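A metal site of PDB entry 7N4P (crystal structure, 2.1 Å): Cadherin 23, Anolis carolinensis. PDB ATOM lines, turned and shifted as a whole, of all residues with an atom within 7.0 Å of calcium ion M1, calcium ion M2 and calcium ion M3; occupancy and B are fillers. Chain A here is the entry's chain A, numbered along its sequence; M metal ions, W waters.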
ATOM      1  N   GLU A  20     -13.539  10.418  16.238  1.00  0.00           N
ATOM      2  CA  GLU A  20     -13.731   8.969  16.087  1.00  0.00           C
ATOM      3  C   GLU A  20     -14.895   8.431  16.948  1.00  0.00           C
ATOM      4  O   GLU A  20     -15.276   7.323  16.664  1.00  0.00           O
ATOM      5  CB  GLU A  20     -12.454   8.216  16.445  1.00  0.00           C
ATOM      6  CG  GLU A  20     -12.114   8.257  17.908  1.00  0.00           C
ATOM      7  CD  GLU A  20     -10.865   7.425  18.196  1.00  0.00           C
ATOM      8  OE1 GLU A  20     -10.730   6.322  17.592  1.00  0.00           O
ATOM      9  OE2 GLU A  20     -10.029   7.898  19.015  1.00  0.00           O
ATOM     10  N   LEU A  69     -15.944   5.013  12.979  1.00  0.00           N
ATOM     11  CA  LEU A  69     -14.564   5.486  12.753  1.00  0.00           C
ATOM     12  C   LEU A  69     -13.668   4.954  13.875  1.00  0.00           C
ATOM     13  O   LEU A  69     -14.160   4.613  14.955  1.00  0.00           O
ATOM     14  CB  LEU A  69     -14.596   7.016  12.747  1.00  0.00           C
ATOM     15  CG  LEU A  69     -15.451   7.636  11.646  1.00  0.00           C
ATOM     16  CD1 LEU A  69     -15.555   9.143  11.860  1.00  0.00           C
ATOM     17  CD2 LEU A  69     -14.879   7.333  10.294  1.00  0.00           C
ATOM     18  N   ASP A  70     -12.383   4.894  13.612  1.00  0.00           N
ATOM     19  CA  ASP A  70     -11.383   4.472  14.635  1.00  0.00           C
ATOM     20  C   ASP A  70     -10.062   5.127  14.232  1.00  0.00           C
ATOM     21  O   ASP A  70      -9.403   4.620  13.282  1.00  0.00           O
ATOM     22  CB  ASP A  70     -11.251   2.964  14.711  1.00  0.00           C
ATOM     23  CG  ASP A  70     -10.168   2.537  15.686  1.00  0.00           C
ATOM     24  OD1 ASP A  70      -9.667   3.372  16.475  1.00  0.00           O
ATOM     25  OD2 ASP A  70      -9.842   1.382  15.641  1.00  0.00           O
ATOM     26  N   ARG A  71      -9.734   6.230  14.877  1.00  0.00           N
ATOM     27  CA  ARG A  71      -8.486   6.927  14.544  1.00  0.00           C
ATOM     28  C   ARG A  71      -7.299   5.974  14.612  1.00  0.00           C
ATOM     29  O   ARG A  71      -6.374   6.245  13.920  1.00  0.00           O
ATOM     30  CB  ARG A  71      -8.206   8.083  15.496  1.00  0.00           C
ATOM     31  CG  ARG A  71      -7.051   8.932  15.009  1.00  0.00           C
ATOM     32  CD  ARG A  71      -6.312   9.601  16.139  1.00  0.00           C
ATOM     33  NE  ARG A  71      -5.688   8.696  17.088  1.00  0.00           N
ATOM     34  CZ  ARG A  71      -4.376   8.456  17.206  1.00  0.00           C
ATOM     35  NH1 ARG A  71      -3.529   8.994  16.362  1.00  0.00           N
ATOM     36  NH2 ARG A  71      -3.929   7.651  18.146  1.00  0.00           N
ATOM     37  N   GLU A  72      -7.333   4.900  15.417  1.00  0.00           N
ATOM     38  CA  GLU A  72      -6.139   4.064  15.655  1.00  0.00           C
ATOM     39  C   GLU A  72      -6.023   3.065  14.506  1.00  0.00           C
ATOM     40  O   GLU A  72      -4.987   2.429  14.372  1.00  0.00           O
ATOM     41  CB  GLU A  72      -6.178   3.309  16.981  1.00  0.00           C
ATOM     42  CG  GLU A  72      -5.772   4.181  18.153  1.00  0.00           C
ATOM     43  CD  GLU A  72      -6.801   5.186  18.664  1.00  0.00           C
ATOM     44  OE1 GLU A  72      -7.993   4.903  18.687  1.00  0.00           O
ATOM     45  OE2 GLU A  72      -6.366   6.278  19.059  1.00  0.00           O
ATOM     46  N   THR A  73      -7.062   2.914  13.710  1.00  0.00           N
ATOM     47  CA  THR A  73      -6.940   2.054  12.512  1.00  0.00           C
ATOM     48  C   THR A  73      -6.768   2.978  11.316  1.00  0.00           C
ATOM     49  O   THR A  73      -5.916   2.718  10.520  1.00  0.00           O
ATOM     50  CB  THR A  73      -8.174   1.164  12.357  1.00  0.00           C
ATOM     51  OG1 THR A  73      -8.560   0.756  13.666  1.00  0.00           O
ATOM     52  CG2 THR A  73      -7.899  -0.037  11.482  1.00  0.00           C
ATOM     53  N   GLY A  99     -10.670  12.614  14.157  1.00  0.00           N
ATOM     54  CA  GLY A  99     -10.164  13.151  15.438  1.00  0.00           C
ATOM     55  C   GLY A  99      -9.994  12.068  16.493  1.00  0.00           C
ATOM     56  O   GLY A  99     -10.907  11.154  16.614  1.00  0.00           O
ATOM     57  N   ASP A 100      -8.898  12.147  17.258  1.00  0.00           N
ATOM     58  CA  ASP A 100      -8.664  11.204  18.387  1.00  0.00           C
ATOM     59  C   ASP A 100      -9.627  11.493  19.543  1.00  0.00           C
ATOM     60  O   ASP A 100      -9.787  12.687  19.882  1.00  0.00           O
ATOM     61  CB  ASP A 100      -7.228  11.254  18.899  1.00  0.00           C
ATOM     62  CG  ASP A 100      -7.012  10.189  19.975  1.00  0.00           C
ATOM     63  OD1 ASP A 100      -7.043   8.985  19.675  1.00  0.00           O
ATOM     64  OD2 ASP A 100      -6.880  10.595  21.106  1.00  0.00           O
ATOM     65  N   VAL A 101     -10.205  10.452  20.156  1.00  0.00           N
ATOM     66  CA  VAL A 101     -10.736  10.523  21.532  1.00  0.00           C
ATOM     67  C   VAL A 101      -9.890   9.567  22.366  1.00  0.00           C
ATOM     68  O   VAL A 101      -9.197   8.655  21.778  1.00  0.00           O
ATOM     69  CB  VAL A 101     -12.230  10.132  21.597  1.00  0.00           C
ATOM     70  CG1 VAL A 101     -12.443   8.655  21.853  1.00  0.00           C
ATOM     71  CG2 VAL A 101     -12.958  10.919  22.683  1.00  0.00           C
ATOM     72  N   ASN A 102      -9.899   9.762  23.688  1.00  0.00           N
ATOM     73  CA  ASN A 102      -9.221   8.841  24.622  1.00  0.00           C
ATOM     74  C   ASN A 102     -10.096   7.610  24.779  1.00  0.00           C
ATOM     75  O   ASN A 102     -10.930   7.620  25.668  1.00  0.00           O
ATOM     76  CB  ASN A 102      -8.936   9.455  25.993  1.00  0.00           C
ATOM     77  CG  ASN A 102      -8.079   8.530  26.841  1.00  0.00           C
ATOM     78  OD1 ASN A 102      -7.161   7.887  26.335  1.00  0.00           O
ATOM     79  ND2 ASN A 102      -8.371   8.493  28.118  1.00  0.00           N
ATOM     80  N   ASP A 103      -9.892   6.585  23.971  1.00  0.00           N
ATOM     81  CA  ASP A 103     -10.793   5.408  23.927  1.00  0.00           C
ATOM     82  C   ASP A 103     -10.022   4.120  24.207  1.00  0.00           C
ATOM     83  O   ASP A 103     -10.599   3.091  23.960  1.00  0.00           O
ATOM     84  CB  ASP A 103     -11.612   5.379  22.621  1.00  0.00           C
ATOM     85  CG  ASP A 103     -10.852   5.351  21.294  1.00  0.00           C
ATOM     86  OD1 ASP A 103      -9.675   5.682  21.277  1.00  0.00           O
ATOM     87  OD2 ASP A 103     -11.484   5.029  20.257  1.00  0.00           O
ATOM     88  N   ASN A 104      -8.751   4.150  24.646  1.00  0.00           N
ATOM     89  CA  ASN A 104      -7.955   2.916  24.948  1.00  0.00           C
ATOM     90  C   ASN A 104      -7.367   3.083  26.355  1.00  0.00           C
ATOM     91  O   ASN A 104      -6.778   4.118  26.612  1.00  0.00           O
ATOM     92  CB  ASN A 104      -6.799   2.691  23.970  1.00  0.00           C
ATOM     93  CG  ASN A 104      -7.296   2.422  22.570  1.00  0.00           C
ATOM     94  OD1 ASN A 104      -7.472   1.276  22.212  1.00  0.00           O
ATOM     95  ND2 ASN A 104      -7.702   3.460  21.849  1.00  0.00           N
ATOM     96  N   ALA A 105      -7.618   2.122  27.229  1.00  0.00           N
ATOM     97  CA  ALA A 105      -6.923   1.923  28.521  1.00  0.00           C
ATOM     98  C   ALA A 105      -5.534   1.408  28.216  1.00  0.00           C
ATOM     99  O   ALA A 105      -5.306   0.799  27.176  1.00  0.00           O
ATOM    100  CB  ALA A 105      -7.660   0.921  29.389  1.00  0.00           C
ATOM    101  N   PRO A 106      -4.551   1.692  29.110  1.00  0.00           N
ATOM    102  CA  PRO A 106      -3.199   1.157  28.931  1.00  0.00           C
ATOM    103  C   PRO A 106      -3.198  -0.377  28.820  1.00  0.00           C
ATOM    104  O   PRO A 106      -4.060  -1.018  29.435  1.00  0.00           O
ATOM    105  CB  PRO A 106      -2.478   1.701  30.165  1.00  0.00           C
ATOM    106  CG  PRO A 106      -3.219   2.978  30.512  1.00  0.00           C
ATOM    107  CD  PRO A 106      -4.667   2.626  30.252  1.00  0.00           C
ATOM    108  N   ASP A 134      -0.101   2.650  25.321  1.00  0.00           N
ATOM    109  CA  ASP A 134      -1.418   3.317  25.166  1.00  0.00           C
ATOM    110  C   ASP A 134      -1.357   4.035  23.838  1.00  0.00           C
ATOM    111  O   ASP A 134      -0.513   4.927  23.667  1.00  0.00           O
ATOM    112  CB  ASP A 134      -1.716   4.247  26.344  1.00  0.00           C
ATOM    113  CG  ASP A 134      -3.145   4.754  26.379  1.00  0.00           C
ATOM    114  OD1 ASP A 134      -3.612   5.191  25.313  1.00  0.00           O
ATOM    115  OD2 ASP A 134      -3.811   4.687  27.479  1.00  0.00           O
ATOM    116  N   PRO A 135      -2.225   3.667  22.881  1.00  0.00           N
ATOM    117  CA  PRO A 135      -2.143   4.161  21.508  1.00  0.00           C
ATOM    118  C   PRO A 135      -2.843   5.501  21.207  1.00  0.00           C
ATOM    119  O   PRO A 135      -2.705   6.015  20.067  1.00  0.00           O
ATOM    120  CB  PRO A 135      -2.829   3.022  20.779  1.00  0.00           C
ATOM    121  CG  PRO A 135      -3.970   2.633  21.711  1.00  0.00           C
ATOM    122  CD  PRO A 135      -3.368   2.736  23.084  1.00  0.00           C
ATOM    123  N   ASP A 136      -3.533   6.069  22.204  1.00  0.00           N
ATOM    124  CA  ASP A 136      -4.289   7.349  22.077  1.00  0.00           C
ATOM    125  C   ASP A 136      -3.298   8.511  21.885  1.00  0.00           C
ATOM    126  O   ASP A 136      -2.197   8.358  22.297  1.00  0.00           O
ATOM    127  CB  ASP A 136      -5.239   7.536  23.264  1.00  0.00           C
ATOM    128  CG  ASP A 136      -6.377   6.519  23.282  1.00  0.00           C
ATOM    129  OD1 ASP A 136      -7.002   6.295  22.193  1.00  0.00           O
ATOM    130  OD2 ASP A 136      -6.583   5.919  24.364  1.00  0.00           O
ATOM    131  N   GLN A 137      -3.762   9.607  21.265  1.00  0.00           N
ATOM    132  CA  GLN A 137      -3.017  10.848  21.013  1.00  0.00           C
ATOM    133  C   GLN A 137      -2.786  11.624  22.313  1.00  0.00           C
ATOM    134  O   GLN A 137      -3.622  11.535  23.201  1.00  0.00           O
ATOM    135  CB  GLN A 137      -3.799  11.679  20.019  1.00  0.00           C
ATOM    136  CG  GLN A 137      -2.924  12.023  18.848  1.00  0.00           C
ATOM    137  CD  GLN A 137      -3.687  12.747  17.764  1.00  0.00           C
ATOM    138  OE1 GLN A 137      -4.731  13.339  17.995  1.00  0.00           O
ATOM    139  NE2 GLN A 137      -3.093  12.726  16.593  1.00  0.00           N
ATOM    140  N   ALA A 139      -1.913  13.453  25.890  1.00  0.00           N
ATOM    141  CA  ALA A 139      -1.947  13.074  27.316  1.00  0.00           C
ATOM    142  C   ALA A 139      -2.683  11.704  27.484  1.00  0.00           C
ATOM    143  O   ALA A 139      -2.212  10.872  28.285  1.00  0.00           O
ATOM    144  CB  ALA A 139      -2.613  14.197  28.085  1.00  0.00           C
ATOM    145  N   GLY A 140      -3.757  11.465  26.710  1.00  0.00           N
ATOM    146  CA  GLY A 140      -4.500  10.191  26.696  1.00  0.00           C
ATOM    147  C   GLY A 140      -3.635   9.011  26.252  1.00  0.00           C
ATOM    148  O   GLY A 140      -4.020   7.842  26.523  1.00  0.00           O
ATOM    149  N   GLY A 141      -2.472   9.279  25.627  1.00  0.00           N
ATOM    150  CA  GLY A 141      -1.526   8.215  25.285  1.00  0.00           C
ATOM    151  C   GLY A 141      -0.336   8.075  26.228  1.00  0.00           C
ATOM    152  O   GLY A 141       0.555   7.240  25.919  1.00  0.00           O
ATOM    153  N   SER A 142      -0.279   8.911  27.276  1.00  0.00           N
ATOM    154  CA  SER A 142       0.826   8.973  28.286  1.00  0.00           C
ATOM    155  C   SER A 142       0.384   8.278  29.567  1.00  0.00           C
ATOM    156  O   SER A 142      -0.656   8.617  30.076  1.00  0.00           O
ATOM    157  CB  SER A 142       1.274  10.381  28.615  1.00  0.00           C
ATOM    158  OG  SER A 142       1.868  10.968  27.487  1.00  0.00           O
ATOM    159  N   ASP A 185      -3.725   6.503  32.090  1.00  0.00           N
ATOM    160  CA  ASP A 185      -3.381   7.542  31.102  1.00  0.00           C
ATOM    161  C   ASP A 185      -3.637   8.927  31.716  1.00  0.00           C
ATOM    162  O   ASP A 185      -4.265   9.024  32.791  1.00  0.00           O
ATOM    163  CB  ASP A 185      -4.010   7.226  29.735  1.00  0.00           C
ATOM    164  CG  ASP A 185      -5.503   7.442  29.588  1.00  0.00           C
ATOM    165  OD1 ASP A 185      -6.037   8.319  30.272  1.00  0.00           O
ATOM    166  OD2 ASP A 185      -6.057   6.785  28.726  1.00  0.00           O
ATOM    167  N   GLN A 186      -3.123   9.965  31.063  1.00  0.00           N
ATOM    168  CA  GLN A 186      -3.093  11.343  31.603  1.00  0.00           C
ATOM    169  C   GLN A 186      -4.143  12.227  30.895  1.00  0.00           C
ATOM    170  O   GLN A 186      -3.933  13.424  30.885  1.00  0.00           O
ATOM    171  CB  GLN A 186      -1.670  11.892  31.480  1.00  0.00           C
ATOM    172  CG  GLN A 186      -0.631  11.011  32.168  1.00  0.00           C
ATOM    173  CD  GLN A 186       0.669  11.768  32.311  1.00  0.00           C
ATOM    174  OE1 GLN A 186       1.734  11.314  31.907  1.00  0.00           O
ATOM    175  NE2 GLN A 186       0.572  12.971  32.853  1.00  0.00           N
ATOM    176  N   ASP A 187      -5.220  11.643  30.360  1.00  0.00           N
ATOM    177  CA  ASP A 187      -6.393  12.402  29.835  1.00  0.00           C
ATOM    178  C   ASP A 187      -6.938  13.269  30.979  1.00  0.00           C
ATOM    179  O   ASP A 187      -7.197  12.720  32.071  1.00  0.00           O
ATOM    180  CB  ASP A 187      -7.513  11.487  29.303  1.00  0.00           C
ATOM    181  CG  ASP A 187      -8.639  12.220  28.572  1.00  0.00           C
ATOM    182  OD1 ASP A 187      -8.423  12.543  27.394  1.00  0.00           O
ATOM    183  OD2 ASP A 187      -9.698  12.500  29.191  1.00  0.00           O
ATOM    184  N   LYS A 190     -11.368  12.173  31.111  1.00  0.00           N
ATOM    185  CA  LYS A 190     -11.732  10.738  31.364  1.00  0.00           C
ATOM    186  C   LYS A 190     -10.479   9.866  31.409  1.00  0.00           C
ATOM    187  O   LYS A 190     -10.238   9.092  30.490  1.00  0.00           O
ATOM    188  CB  LYS A 190     -12.740  10.234  30.312  1.00  0.00           C
ATOM    189  CG  LYS A 190     -12.122   9.725  29.002  1.00  0.00           C
ATOM    190  CD  LYS A 190     -13.120   9.404  27.886  1.00  0.00           C
ATOM    191  CE  LYS A 190     -13.950  10.581  27.378  1.00  0.00           C
ATOM    192  NZ  LYS A 190     -14.845  10.190  26.254  1.00  0.00           N
ATOM    193  N   PRO A 191      -9.630   9.921  32.456  1.00  0.00           N
ATOM    194  CA  PRO A 191      -8.391   9.153  32.410  1.00  0.00           C
ATOM    195  C   PRO A 191      -8.811   7.682  32.431  1.00  0.00           C
ATOM    196  O   PRO A 191      -9.771   7.426  33.087  1.00  0.00           O
ATOM    197  CB  PRO A 191      -7.660   9.545  33.683  1.00  0.00           C
ATOM    198  CG  PRO A 191      -8.787   9.955  34.613  1.00  0.00           C
ATOM    199  CD  PRO A 191      -9.814  10.625  33.724  1.00  0.00           C
ATOM    200  N   LEU A 192      -8.173   6.789  31.671  1.00  0.00           N
ATOM    201  CA  LEU A 192      -8.476   5.345  31.719  1.00  0.00           C
ATOM    202  C   LEU A 192      -7.301   4.622  32.367  1.00  0.00           C
ATOM    203  O   LEU A 192      -6.157   5.105  32.221  1.00  0.00           O
ATOM    204  CB  LEU A 192      -8.742   4.836  30.307  1.00  0.00           C
ATOM    205  CG  LEU A 192      -9.878   5.571  29.586  1.00  0.00           C
ATOM    206  CD1 LEU A 192     -10.108   4.998  28.200  1.00  0.00           C
ATOM    207  CD2 LEU A 192     -11.162   5.540  30.405  1.00  0.00           C
HETATM  208 CA    CA M   1      -5.653   6.119  26.533  1.00  0.00          CA
HETATM  209 CA    CA M   2      -8.172   7.114  20.292  1.00  0.00          CA
HETATM  210 CA    CA M   3     -10.198   4.309  18.517  1.00  0.00          CA
HETATM  211  O   HOH W   1     -12.116   3.363  18.145  1.00  0.00           O
HETATM  212  O   HOH W   2      -9.541   2.394  19.600  1.00  0.00           O
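The side-chain carboxylate (OD2) of Asp 100 sits at hydrogen-bond distance from the backbone NH (N) of Gln 137, 3.3 Å away. The backbone NH (N) of Arg 71 lies close to the side-chain carboxylate (OE1) of Glu 20, at 2.9 Å. The backbone NH (N) of Glu 20 sits at hydrogen-bond distance from the backbone carbonyl oxygen (O) of Gly 99, 2.8 Å away. ND2 of Asn 104 sits close to OE1 of Glu 72 (3.5 Å). The side-chain carboxylate of Glu 72 lies close to the guanidinium group of Arg 71 (2.9 Å). OG1 of Thr 73 is in hydrogen-bond range of OD2 of Asp 70 (2.4 Å). The side-chain carboxylate (OD1) of Asp 185 sits close to the backbone NH (N) of Asp 187 (3.4 Å). The side-chain amide nitrogen (ND2) of Asn 102 sits at hydrogen-bond distance from the backbone carbonyl oxygen (O) of Lys 190 (3.1 Å).
Within 4 Å of calcium ion M1: Asn 102, Asn 104, Asp 134, Asp 136, Gly 140 and Asp 185.
The nearest printed residue that does not touch calcium ion M2 is Arg 71 (4.4 Å).
Of the 28 residues printed, 4 come within 4 Å of calcium ion M3.
Calcium ion M1 is bound by the backbone carbonyl oxygen (O) of Asn 104, the side-chain carboxylate (OD2) of Asp 185, the side-chain amide oxygen (OD1) of Asn 102, the side-chain carboxylate (OD2) of Asp 136, the backbone carbonyl oxygen (O) of Gly 140, the side-chain carboxylate (OD2) of Asp 134 and the side-chain carboxylate (OD1) of Asp 134. Calcium ion M1 has seven donor atoms within binding distance.
Calcium ion M2 is bound by the side-chain carboxylate (OD1) of Asp 100, the side-chain carboxylate (OD1) of Asp 103, the side-chain carboxylate (OE2) of Glu 72, the backbone carbonyl oxygen (O) of Val 101, the side-chain carboxylate (OD1) of Asp 136, the side-chain carboxylate (OE2) of Glu 20 and the side-chain carboxylate (OE1) of Glu 72. Calcium ion M2 has seven donor atoms within binding distance.
Calcium ion M3 is bound by water W1 (2.2 Å), OE1 of Glu 20 (2.3 Å), OD2 of Asp 103 (2.3 Å), OE1 of Glu 72 (2.3 Å), water W2 (2.3 Å) and OD1 of Asp 70 (2.3 Å). Slightly farther from calcium ion M3 lies OD1 of Asp 103 (3.1 Å).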
